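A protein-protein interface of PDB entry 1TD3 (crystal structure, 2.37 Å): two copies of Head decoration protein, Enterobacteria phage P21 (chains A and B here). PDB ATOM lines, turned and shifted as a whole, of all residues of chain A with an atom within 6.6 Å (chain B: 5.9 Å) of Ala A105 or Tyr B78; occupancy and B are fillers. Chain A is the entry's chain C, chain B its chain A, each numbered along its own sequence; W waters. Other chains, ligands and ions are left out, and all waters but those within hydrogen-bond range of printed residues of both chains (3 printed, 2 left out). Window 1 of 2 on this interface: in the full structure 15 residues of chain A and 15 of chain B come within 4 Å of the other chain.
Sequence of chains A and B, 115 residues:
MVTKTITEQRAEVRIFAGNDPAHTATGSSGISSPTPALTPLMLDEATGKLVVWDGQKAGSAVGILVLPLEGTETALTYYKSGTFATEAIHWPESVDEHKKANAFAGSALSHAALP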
ATOM      1  N   ALA A  58      -0.378  21.321  16.421  1.00  0.00           N
ATOM      2  CA  ALA A  58       0.699  22.142  16.943  1.00  0.00           C
ATOM      3  C   ALA A  58       1.894  21.857  16.035  1.00  0.00           C
ATOM      4  O   ALA A  58       2.109  20.711  15.635  1.00  0.00           O
ATOM      5  CB  ALA A  58       1.022  21.734  18.355  1.00  0.00           C
ATOM      6  N   GLY A  59       2.657  22.894  15.690  1.00  0.00           N
ATOM      7  CA  GLY A  59       3.828  22.695  14.847  1.00  0.00           C
ATOM      8  C   GLY A  59       3.535  22.739  13.361  1.00  0.00           C
ATOM      9  O   GLY A  59       4.439  22.586  12.534  1.00  0.00           O
ATOM     10  N   SER A  60       2.270  22.965  13.020  1.00  0.00           N
ATOM     11  CA  SER A  60       1.837  23.016  11.626  1.00  0.00           C
ATOM     12  C   SER A  60       1.982  24.418  11.020  1.00  0.00           C
ATOM     13  O   SER A  60       2.182  24.557   9.815  1.00  0.00           O
ATOM     14  CB  SER A  60       0.365  22.547  11.519  1.00  0.00           C
ATOM     15  OG  SER A  60      -0.143  22.739  10.214  1.00  0.00           O
ATOM     16  N   ALA A  61       1.849  25.453  11.842  1.00  0.00           N
ATOM     17  CA  ALA A  61       1.980  26.838  11.355  1.00  0.00           C
ATOM     18  C   ALA A  61       3.451  27.052  10.967  1.00  0.00           C
ATOM     19  O   ALA A  61       4.326  27.026  11.817  1.00  0.00           O
ATOM     20  CB  ALA A  61       1.558  27.825  12.446  1.00  0.00           C
ATOM     21  N   ALA A 101      -0.005  27.881  21.594  1.00  0.00           N
ATOM     22  CA  ALA A 101       1.308  28.188  22.131  1.00  0.00           C
ATOM     23  C   ALA A 101       2.436  27.496  21.370  1.00  0.00           C
ATOM     24  O   ALA A 101       3.513  28.069  21.193  1.00  0.00           O
ATOM     25  CB  ALA A 101       1.358  27.813  23.591  1.00  0.00           C
ATOM     26  N   ASN A 102       2.189  26.270  20.917  1.00  0.00           N
ATOM     27  CA  ASN A 102       3.195  25.508  20.181  1.00  0.00           C
ATOM     28  C   ASN A 102       2.927  25.494  18.687  1.00  0.00           C
ATOM     29  O   ASN A 102       3.410  24.620  17.965  1.00  0.00           O
ATOM     30  CB  ASN A 102       3.269  24.064  20.694  1.00  0.00           C
ATOM     31  CG  ASN A 102       3.625  23.989  22.160  1.00  0.00           C
ATOM     32  OD1 ASN A 102       4.336  24.848  22.676  1.00  0.00           O
ATOM     33  ND2 ASN A 102       3.145  22.948  22.838  1.00  0.00           N
ATOM     34  N   ALA A 103       2.172  26.472  18.214  1.00  0.00           N
ATOM     35  CA  ALA A 103       1.852  26.536  16.802  1.00  0.00           C
ATOM     36  C   ALA A 103       3.048  26.450  15.857  1.00  0.00           C
ATOM     37  O   ALA A 103       2.992  25.745  14.831  1.00  0.00           O
ATOM     38  CB  ALA A 103       1.078  27.797  16.515  1.00  0.00           C
ATOM     39  N   PHE A 104       4.122  27.177  16.176  1.00  0.00           N
ATOM     40  CA  PHE A 104       5.285  27.198  15.290  1.00  0.00           C
ATOM     41  C   PHE A 104       6.419  26.297  15.724  1.00  0.00           C
ATOM     42  O   PHE A 104       7.461  26.275  15.081  1.00  0.00           O
ATOM     43  CB  PHE A 104       5.831  28.625  15.135  1.00  0.00           C
ATOM     44  CG  PHE A 104       4.774  29.667  14.912  1.00  0.00           C
ATOM     45  CD1 PHE A 104       4.249  30.379  15.985  1.00  0.00           C
ATOM     46  CD2 PHE A 104       4.305  29.939  13.632  1.00  0.00           C
ATOM     47  CE1 PHE A 104       3.272  31.352  15.787  1.00  0.00           C
ATOM     48  CE2 PHE A 104       3.326  30.907  13.422  1.00  0.00           C
ATOM     49  CZ  PHE A 104       2.807  31.617  14.503  1.00  0.00           C
ATOM     50  N   ALA A 105       6.223  25.558  16.806  1.00  0.00           N
ATOM     51  CA  ALA A 105       7.268  24.674  17.291  1.00  0.00           C
ATOM     52  C   ALA A 105       7.788  23.829  16.134  1.00  0.00           C
ATOM     53  O   ALA A 105       7.017  23.145  15.462  1.00  0.00           O
ATOM     54  CB  ALA A 105       6.731  23.787  18.391  1.00  0.00           C
ATOM     55  N   GLY A 106       9.090  23.902  15.885  1.00  0.00           N
ATOM     56  CA  GLY A 106       9.656  23.119  14.801  1.00  0.00           C
ATOM     57  C   GLY A 106      10.232  24.013  13.736  1.00  0.00           C
ATOM     58  O   GLY A 106      11.183  23.627  13.053  1.00  0.00           O
ATOM     59  N   SER A 107       9.651  25.201  13.581  1.00  0.00           N
ATOM     60  CA  SER A 107      10.149  26.157  12.594  1.00  0.00           C
ATOM     61  C   SER A 107      11.092  27.124  13.317  1.00  0.00           C
ATOM     62  O   SER A 107      11.478  26.875  14.463  1.00  0.00           O
ATOM     63  CB  SER A 107       8.992  26.944  11.988  1.00  0.00           C
ATOM     64  OG  SER A 107       8.429  27.801  12.971  1.00  0.00           O
ATOM     65  N   LEU A 109      10.207  30.160  13.899  1.00  0.00           N
ATOM     66  CA  LEU A 109       9.292  31.117  14.505  1.00  0.00           C
ATOM     67  C   LEU A 109       8.937  30.727  15.926  1.00  0.00           C
ATOM     68  O   LEU A 109       9.147  29.595  16.347  1.00  0.00           O
ATOM     69  CB  LEU A 109       8.014  31.198  13.679  1.00  0.00           C
ATOM     70  CG  LEU A 109       8.172  31.739  12.257  1.00  0.00           C
ATOM     71  CD1 LEU A 109       6.967  31.360  11.411  1.00  0.00           C
ATOM     72  CD2 LEU A 109       8.333  33.238  12.323  1.00  0.00           C
ATOM     73  N   SER A 110       8.412  31.683  16.676  1.00  0.00           N
ATOM     74  CA  SER A 110       7.990  31.439  18.044  1.00  0.00           C
ATOM     75  C   SER A 110       7.238  32.679  18.455  1.00  0.00           C
ATOM     76  O   SER A 110       7.278  33.686  17.755  1.00  0.00           O
ATOM     77  CB  SER A 110       9.191  31.187  18.962  1.00  0.00           C
ATOM     78  OG  SER A 110      10.079  32.286  18.987  1.00  0.00           O
ATOM     79  N   HIS B  23      18.877  30.579  20.037  1.00  0.00           N
ATOM     80  CA  HIS B  23      17.753  31.375  20.517  1.00  0.00           C
ATOM     81  C   HIS B  23      16.824  30.436  21.266  1.00  0.00           C
ATOM     82  O   HIS B  23      16.836  29.231  21.025  1.00  0.00           O
ATOM     83  CB  HIS B  23      17.002  32.019  19.346  1.00  0.00           C
ATOM     84  CG  HIS B  23      17.840  32.961  18.539  1.00  0.00           C
ATOM     85  ND1 HIS B  23      18.099  32.769  17.198  1.00  0.00           N
ATOM     86  CD2 HIS B  23      18.483  34.099  18.887  1.00  0.00           C
ATOM     87  CE1 HIS B  23      18.866  33.748  16.756  1.00  0.00           C
ATOM     88  NE2 HIS B  23      19.114  34.568  17.761  1.00  0.00           N
ATOM     89  N   THR B  24      16.023  30.988  22.172  1.00  0.00           N
ATOM     90  CA  THR B  24      15.091  30.195  22.950  1.00  0.00           C
ATOM     91  C   THR B  24      13.646  30.588  22.652  1.00  0.00           C
ATOM     92  O   THR B  24      13.373  31.598  21.997  1.00  0.00           O
ATOM     93  CB  THR B  24      15.308  30.392  24.443  1.00  0.00           C
ATOM     94  OG1 THR B  24      14.999  31.752  24.781  1.00  0.00           O
ATOM     95  CG2 THR B  24      16.744  30.059  24.825  1.00  0.00           C
ATOM     96  N   ALA B  25      12.723  29.783  23.164  1.00  0.00           N
ATOM     97  CA  ALA B  25      11.304  30.017  22.980  1.00  0.00           C
ATOM     98  C   ALA B  25      10.563  29.283  24.097  1.00  0.00           C
ATOM     99  O   ALA B  25      11.138  28.435  24.784  1.00  0.00           O
ATOM    100  CB  ALA B  25      10.872  29.477  21.622  1.00  0.00           C
ATOM    101  N   THR B  26       9.295  29.615  24.285  1.00  0.00           N
ATOM    102  CA  THR B  26       8.482  28.955  25.299  1.00  0.00           C
ATOM    103  C   THR B  26       7.352  28.198  24.599  1.00  0.00           C
ATOM    104  O   THR B  26       7.059  28.462  23.428  1.00  0.00           O
ATOM    105  CB  THR B  26       7.880  29.982  26.265  1.00  0.00           C
ATOM    106  OG1 THR B  26       7.324  31.066  25.511  1.00  0.00           O
ATOM    107  CG2 THR B  26       8.955  30.523  27.198  1.00  0.00           C
ATOM    108  N   GLY B  27       6.740  27.261  25.320  1.00  0.00           N
ATOM    109  CA  GLY B  27       5.639  26.472  24.783  1.00  0.00           C
ATOM    110  C   GLY B  27       4.947  25.636  25.857  1.00  0.00           C
ATOM    111  O   GLY B  27       5.528  25.393  26.924  1.00  0.00           O
ATOM    112  N   LEU B  41      13.206  17.535  22.646  1.00  0.00           N
ATOM    113  CA  LEU B  41      11.756  17.605  22.779  1.00  0.00           C
ATOM    114  C   LEU B  41      11.037  17.366  21.461  1.00  0.00           C
ATOM    115  O   LEU B  41      11.591  17.609  20.380  1.00  0.00           O
ATOM    116  CB  LEU B  41      11.347  18.975  23.320  1.00  0.00           C
ATOM    117  CG  LEU B  41      11.898  19.388  24.687  1.00  0.00           C
ATOM    118  CD1 LEU B  41      11.366  20.774  25.042  1.00  0.00           C
ATOM    119  CD2 LEU B  41      11.478  18.377  25.741  1.00  0.00           C
ATOM    120  N   LEU B  43       6.706  17.189  19.722  1.00  0.00           N
ATOM    121  CA  LEU B  43       5.318  17.566  19.955  1.00  0.00           C
ATOM    122  C   LEU B  43       4.471  16.297  20.140  1.00  0.00           C
ATOM    123  O   LEU B  43       4.741  15.263  19.522  1.00  0.00           O
ATOM    124  CB  LEU B  43       4.768  18.370  18.770  1.00  0.00           C
ATOM    125  CG  LEU B  43       5.284  19.798  18.553  1.00  0.00           C
ATOM    126  CD1 LEU B  43       4.838  20.309  17.195  1.00  0.00           C
ATOM    127  CD2 LEU B  43       4.763  20.698  19.662  1.00  0.00           C
ATOM    128  N   LEU B  50       4.421  19.826  24.229  1.00  0.00           N
ATOM    129  CA  LEU B  50       5.790  19.381  24.076  1.00  0.00           C
ATOM    130  C   LEU B  50       6.120  18.334  25.132  1.00  0.00           C
ATOM    131  O   LEU B  50       5.768  18.468  26.302  1.00  0.00           O
ATOM    132  CB  LEU B  50       6.748  20.572  24.202  1.00  0.00           C
ATOM    133  CG  LEU B  50       6.727  21.525  23.003  1.00  0.00           C
ATOM    134  CD1 LEU B  50       7.310  22.883  23.389  1.00  0.00           C
ATOM    135  CD2 LEU B  50       7.509  20.882  21.858  1.00  0.00           C
ATOM    136  N   VAL B  62      11.901  18.921  18.045  1.00  0.00           N
ATOM    137  CA  VAL B  62      11.754  20.321  17.644  1.00  0.00           C
ATOM    138  C   VAL B  62      12.365  21.340  18.606  1.00  0.00           C
ATOM    139  O   VAL B  62      12.192  22.545  18.429  1.00  0.00           O
ATOM    140  CB  VAL B  62      10.268  20.669  17.472  1.00  0.00           C
ATOM    141  CG1 VAL B  62       9.637  19.776  16.414  1.00  0.00           C
ATOM    142  CG2 VAL B  62       9.567  20.496  18.780  1.00  0.00           C
ATOM    143  N   GLY B  63      13.063  20.853  19.626  1.00  0.00           N
ATOM    144  CA  GLY B  63      13.678  21.744  20.587  1.00  0.00           C
ATOM    145  C   GLY B  63      14.487  21.018  21.646  1.00  0.00           C
ATOM    146  O   GLY B  63      14.430  19.787  21.775  1.00  0.00           O
ATOM    147  N   ILE B  64      15.277  21.787  22.386  1.00  0.00           N
ATOM    148  CA  ILE B  64      16.086  21.237  23.458  1.00  0.00           C
ATOM    149  C   ILE B  64      15.773  22.026  24.726  1.00  0.00           C
ATOM    150  O   ILE B  64      15.855  23.260  24.751  1.00  0.00           O
ATOM    151  CB  ILE B  64      17.563  21.343  23.141  1.00  0.00           C
ATOM    152  CG1 ILE B  64      17.862  20.584  21.841  1.00  0.00           C
ATOM    153  CG2 ILE B  64      18.370  20.819  24.321  1.00  0.00           C
ATOM    154  CD1 ILE B  64      19.278  20.784  21.309  1.00  0.00           C
ATOM    155  N   LEU B  65      15.390  21.297  25.767  1.00  0.00           N
ATOM    156  CA  LEU B  65      15.020  21.881  27.042  1.00  0.00           C
ATOM    157  C   LEU B  65      16.151  22.732  27.619  1.00  0.00           C
ATOM    158  O   LEU B  65      17.279  22.262  27.753  1.00  0.00           O
ATOM    159  CB  LEU B  65      14.645  20.757  28.015  1.00  0.00           C
ATOM    160  CG  LEU B  65      14.083  21.175  29.368  1.00  0.00           C
ATOM    161  CD1 LEU B  65      12.770  21.944  29.182  1.00  0.00           C
ATOM    162  CD2 LEU B  65      13.865  19.941  30.217  1.00  0.00           C
ATOM    163  N   VAL B  66      15.853  23.983  27.956  1.00  0.00           N
ATOM    164  CA  VAL B  66      16.877  24.869  28.521  1.00  0.00           C
ATOM    165  C   VAL B  66      17.125  24.537  29.992  1.00  0.00           C
ATOM    166  O   VAL B  66      18.235  24.180  30.378  1.00  0.00           O
ATOM    167  CB  VAL B  66      16.470  26.352  28.420  1.00  0.00           C
ATOM    168  CG1 VAL B  66      17.591  27.230  28.956  1.00  0.00           C
ATOM    169  CG2 VAL B  66      16.169  26.713  26.982  1.00  0.00           C
ATOM    170  N   LEU B  76       7.245  25.478  29.381  1.00  0.00           N
ATOM    171  CA  LEU B  76       8.672  25.168  29.405  1.00  0.00           C
ATOM    172  C   LEU B  76       9.440  26.071  28.438  1.00  0.00           C
ATOM    173  O   LEU B  76       8.852  26.718  27.569  1.00  0.00           O
ATOM    174  CB  LEU B  76       8.902  23.694  29.057  1.00  0.00           C
ATOM    175  CG  LEU B  76       8.501  23.135  27.683  1.00  0.00           C
ATOM    176  CD1 LEU B  76       9.488  23.579  26.612  1.00  0.00           C
ATOM    177  CD2 LEU B  76       8.502  21.617  27.756  1.00  0.00           C
ATOM    178  N   THR B  77      10.757  26.106  28.602  1.00  0.00           N
ATOM    179  CA  THR B  77      11.632  26.933  27.766  1.00  0.00           C
ATOM    180  C   THR B  77      12.595  26.043  26.995  1.00  0.00           C
ATOM    181  O   THR B  77      13.222  25.148  27.564  1.00  0.00           O
ATOM    182  CB  THR B  77      12.461  27.919  28.639  1.00  0.00           C
ATOM    183  OG1 THR B  77      11.566  28.749  29.390  1.00  0.00           O
ATOM    184  CG2 THR B  77      13.374  28.796  27.765  1.00  0.00           C
ATOM    185  N   TYR B  78      12.726  26.291  25.699  1.00  0.00           N
ATOM    186  CA  TYR B  78      13.622  25.471  24.901  1.00  0.00           C
ATOM    187  C   TYR B  78      14.388  26.249  23.837  1.00  0.00           C
ATOM    188  O   TYR B  78      13.975  27.335  23.413  1.00  0.00           O
ATOM    189  CB  TYR B  78      12.830  24.341  24.221  1.00  0.00           C
ATOM    190  CG  TYR B  78      11.754  24.819  23.263  1.00  0.00           C
ATOM    191  CD1 TYR B  78      10.515  25.267  23.727  1.00  0.00           C
ATOM    192  CD2 TYR B  78      11.965  24.793  21.886  1.00  0.00           C
ATOM    193  CE1 TYR B  78       9.504  25.674  22.835  1.00  0.00           C
ATOM    194  CE2 TYR B  78      10.965  25.190  20.995  1.00  0.00           C
ATOM    195  CZ  TYR B  78       9.741  25.627  21.473  1.00  0.00           C
ATOM    196  OH  TYR B  78       8.757  26.001  20.567  1.00  0.00           O
ATOM    197  N   TYR B  79      15.508  25.673  23.412  1.00  0.00           N
ATOM    198  CA  TYR B  79      16.323  26.262  22.361  1.00  0.00           C
ATOM    199  C   TYR B  79      15.654  25.922  21.027  1.00  0.00           C
ATOM    200  O   TYR B  79      15.350  24.753  20.761  1.00  0.00           O
ATOM    201  CB  TYR B  79      17.734  25.667  22.378  1.00  0.00           C
ATOM    202  CG  TYR B  79      18.528  25.922  23.643  1.00  0.00           C
ATOM    203  CD1 TYR B  79      18.747  24.901  24.573  1.00  0.00           C
ATOM    204  CD2 TYR B  79      19.114  27.168  23.883  1.00  0.00           C
ATOM    205  CE1 TYR B  79      19.538  25.109  25.701  1.00  0.00           C
ATOM    206  CE2 TYR B  79      19.912  27.391  25.016  1.00  0.00           C
ATOM    207  CZ  TYR B  79      20.122  26.363  25.913  1.00  0.00           C
ATOM    208  OH  TYR B  79      20.939  26.579  27.000  1.00  0.00           O
ATOM    209  N   LYS B  80      15.427  26.926  20.189  1.00  0.00           N
ATOM    210  CA  LYS B  80      14.795  26.704  18.908  1.00  0.00           C
ATOM    211  C   LYS B  80      15.769  26.779  17.751  1.00  0.00           C
ATOM    212  O   LYS B  80      15.369  26.625  16.599  1.00  0.00           O
ATOM    213  CB  LYS B  80      13.667  27.715  18.679  1.00  0.00           C
ATOM    214  CG  LYS B  80      14.128  29.167  18.524  1.00  0.00           C
ATOM    215  CD  LYS B  80      12.968  30.041  18.042  1.00  0.00           C
ATOM    216  CE  LYS B  80      13.369  31.486  17.870  1.00  0.00           C
ATOM    217  NZ  LYS B  80      12.261  32.298  17.297  1.00  0.00           N
HETATM  218  O   HOH W   1      11.773  24.612  17.092  1.00  0.00           O
HETATM  219  O   HOH W   2      13.469  25.415  15.053  1.00  0.00           O
HETATM  220  O   HOH W   3      11.048  32.878  21.524  1.00  0.00           O
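The side-chain amino group of Lys B80 lies within hydrogen-bond range of the side-chain hydroxyl of Ser A110 (2.8 Å).
Ala A105 touches just these residues of chain B: Leu B43 and Tyr B78.
Tyr B78 touches just one residue of chain A: Ala A105 (3.7 Å).
Printed residues of chain B within 4 Å of Ala A58: Leu B43 (3.2 Å).
Printed residues of chain A within 4 Å of Leu B43: Ala A58 (3.2 Å), Gly A59 (3.5 Å), Asn A102 (3.8 Å) and Ala A105 (3.9 Å).
Printed residues of chain B within 4 Å of Leu A109: Lys B80.
Leu B41 touches none of the printed residues of chain A.
Val B66 touches none of the printed residues of chain A.
The nearest residue of chain B that does not touch Ala A105 is Val B62 (4.2 Å).
No position is printed for both chains.
Of the 11 pairs that touch across the chains among the printed residues, none has its exchanged pair printed and touching as well.
Among the printed residues, merely in contact across the chains: Ala A58 with Leu B43, Gly A59 with Leu B43, Asn A102 with Gly B27, Asn A102 with Leu B43, Asn A102 with Leu B50, Ala A105 with Leu B43, Ala A105 with Tyr B78, Gly A106 with Val B62, Leu A109 with Lys B80 and Ser A110 with Ala B25.
The backbone carbonyl oxygen of His B23 sits at hydrogen-bond distance from the backbone NH of Lys B80.
The backbone NH of Leu B76 is in hydrogen-bond range of the backbone carbonyl oxygen of Gly B27.
The backbone NH (N) of Gly A59 lies within hydrogen-bond range of the backbone carbonyl oxygen (O) of Asn A102 (3.0 Å).
The backbone NH of Ala B25 sits at hydrogen-bond distance from the backbone carbonyl oxygen of Tyr B78, 2.8 Å away.
O of Ala A103 sits at hydrogen-bond distance from N of Gly A59, at 3.0 Å.
The backbone NH (N) of Leu A109 sits at hydrogen-bond distance from the side-chain hydroxyl (OG) of Ser A107.
Hydrophobic or aromatic side chains of chain A within 4 Å of the printed part of chain B: Ala A105.
Hydrophobic or aromatic side chains of chain B that line the printed part of chain A: Ala B25, Leu B43, Leu B50, Val B62 and Tyr B78.
Among the printed residues, no Asp or Glu carboxylate lies within 4 Å of a Lys or Arg side-chain nitrogen of the other chain.
Water W1 lies within hydrogen-bond range of O of Val B62, N of Gly A106 and O of Ser A107.
Water W2 lies within hydrogen-bond range of O of Ser A107 (2.5 Å) and O of Lys B80 (2.7 Å).
Water W3 lies within hydrogen-bond range of the backbone carbonyl oxygen (O) of Thr B24 (2.7 Å) and the side-chain hydroxyl (OG) of Ser A110 (2.8 Å).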
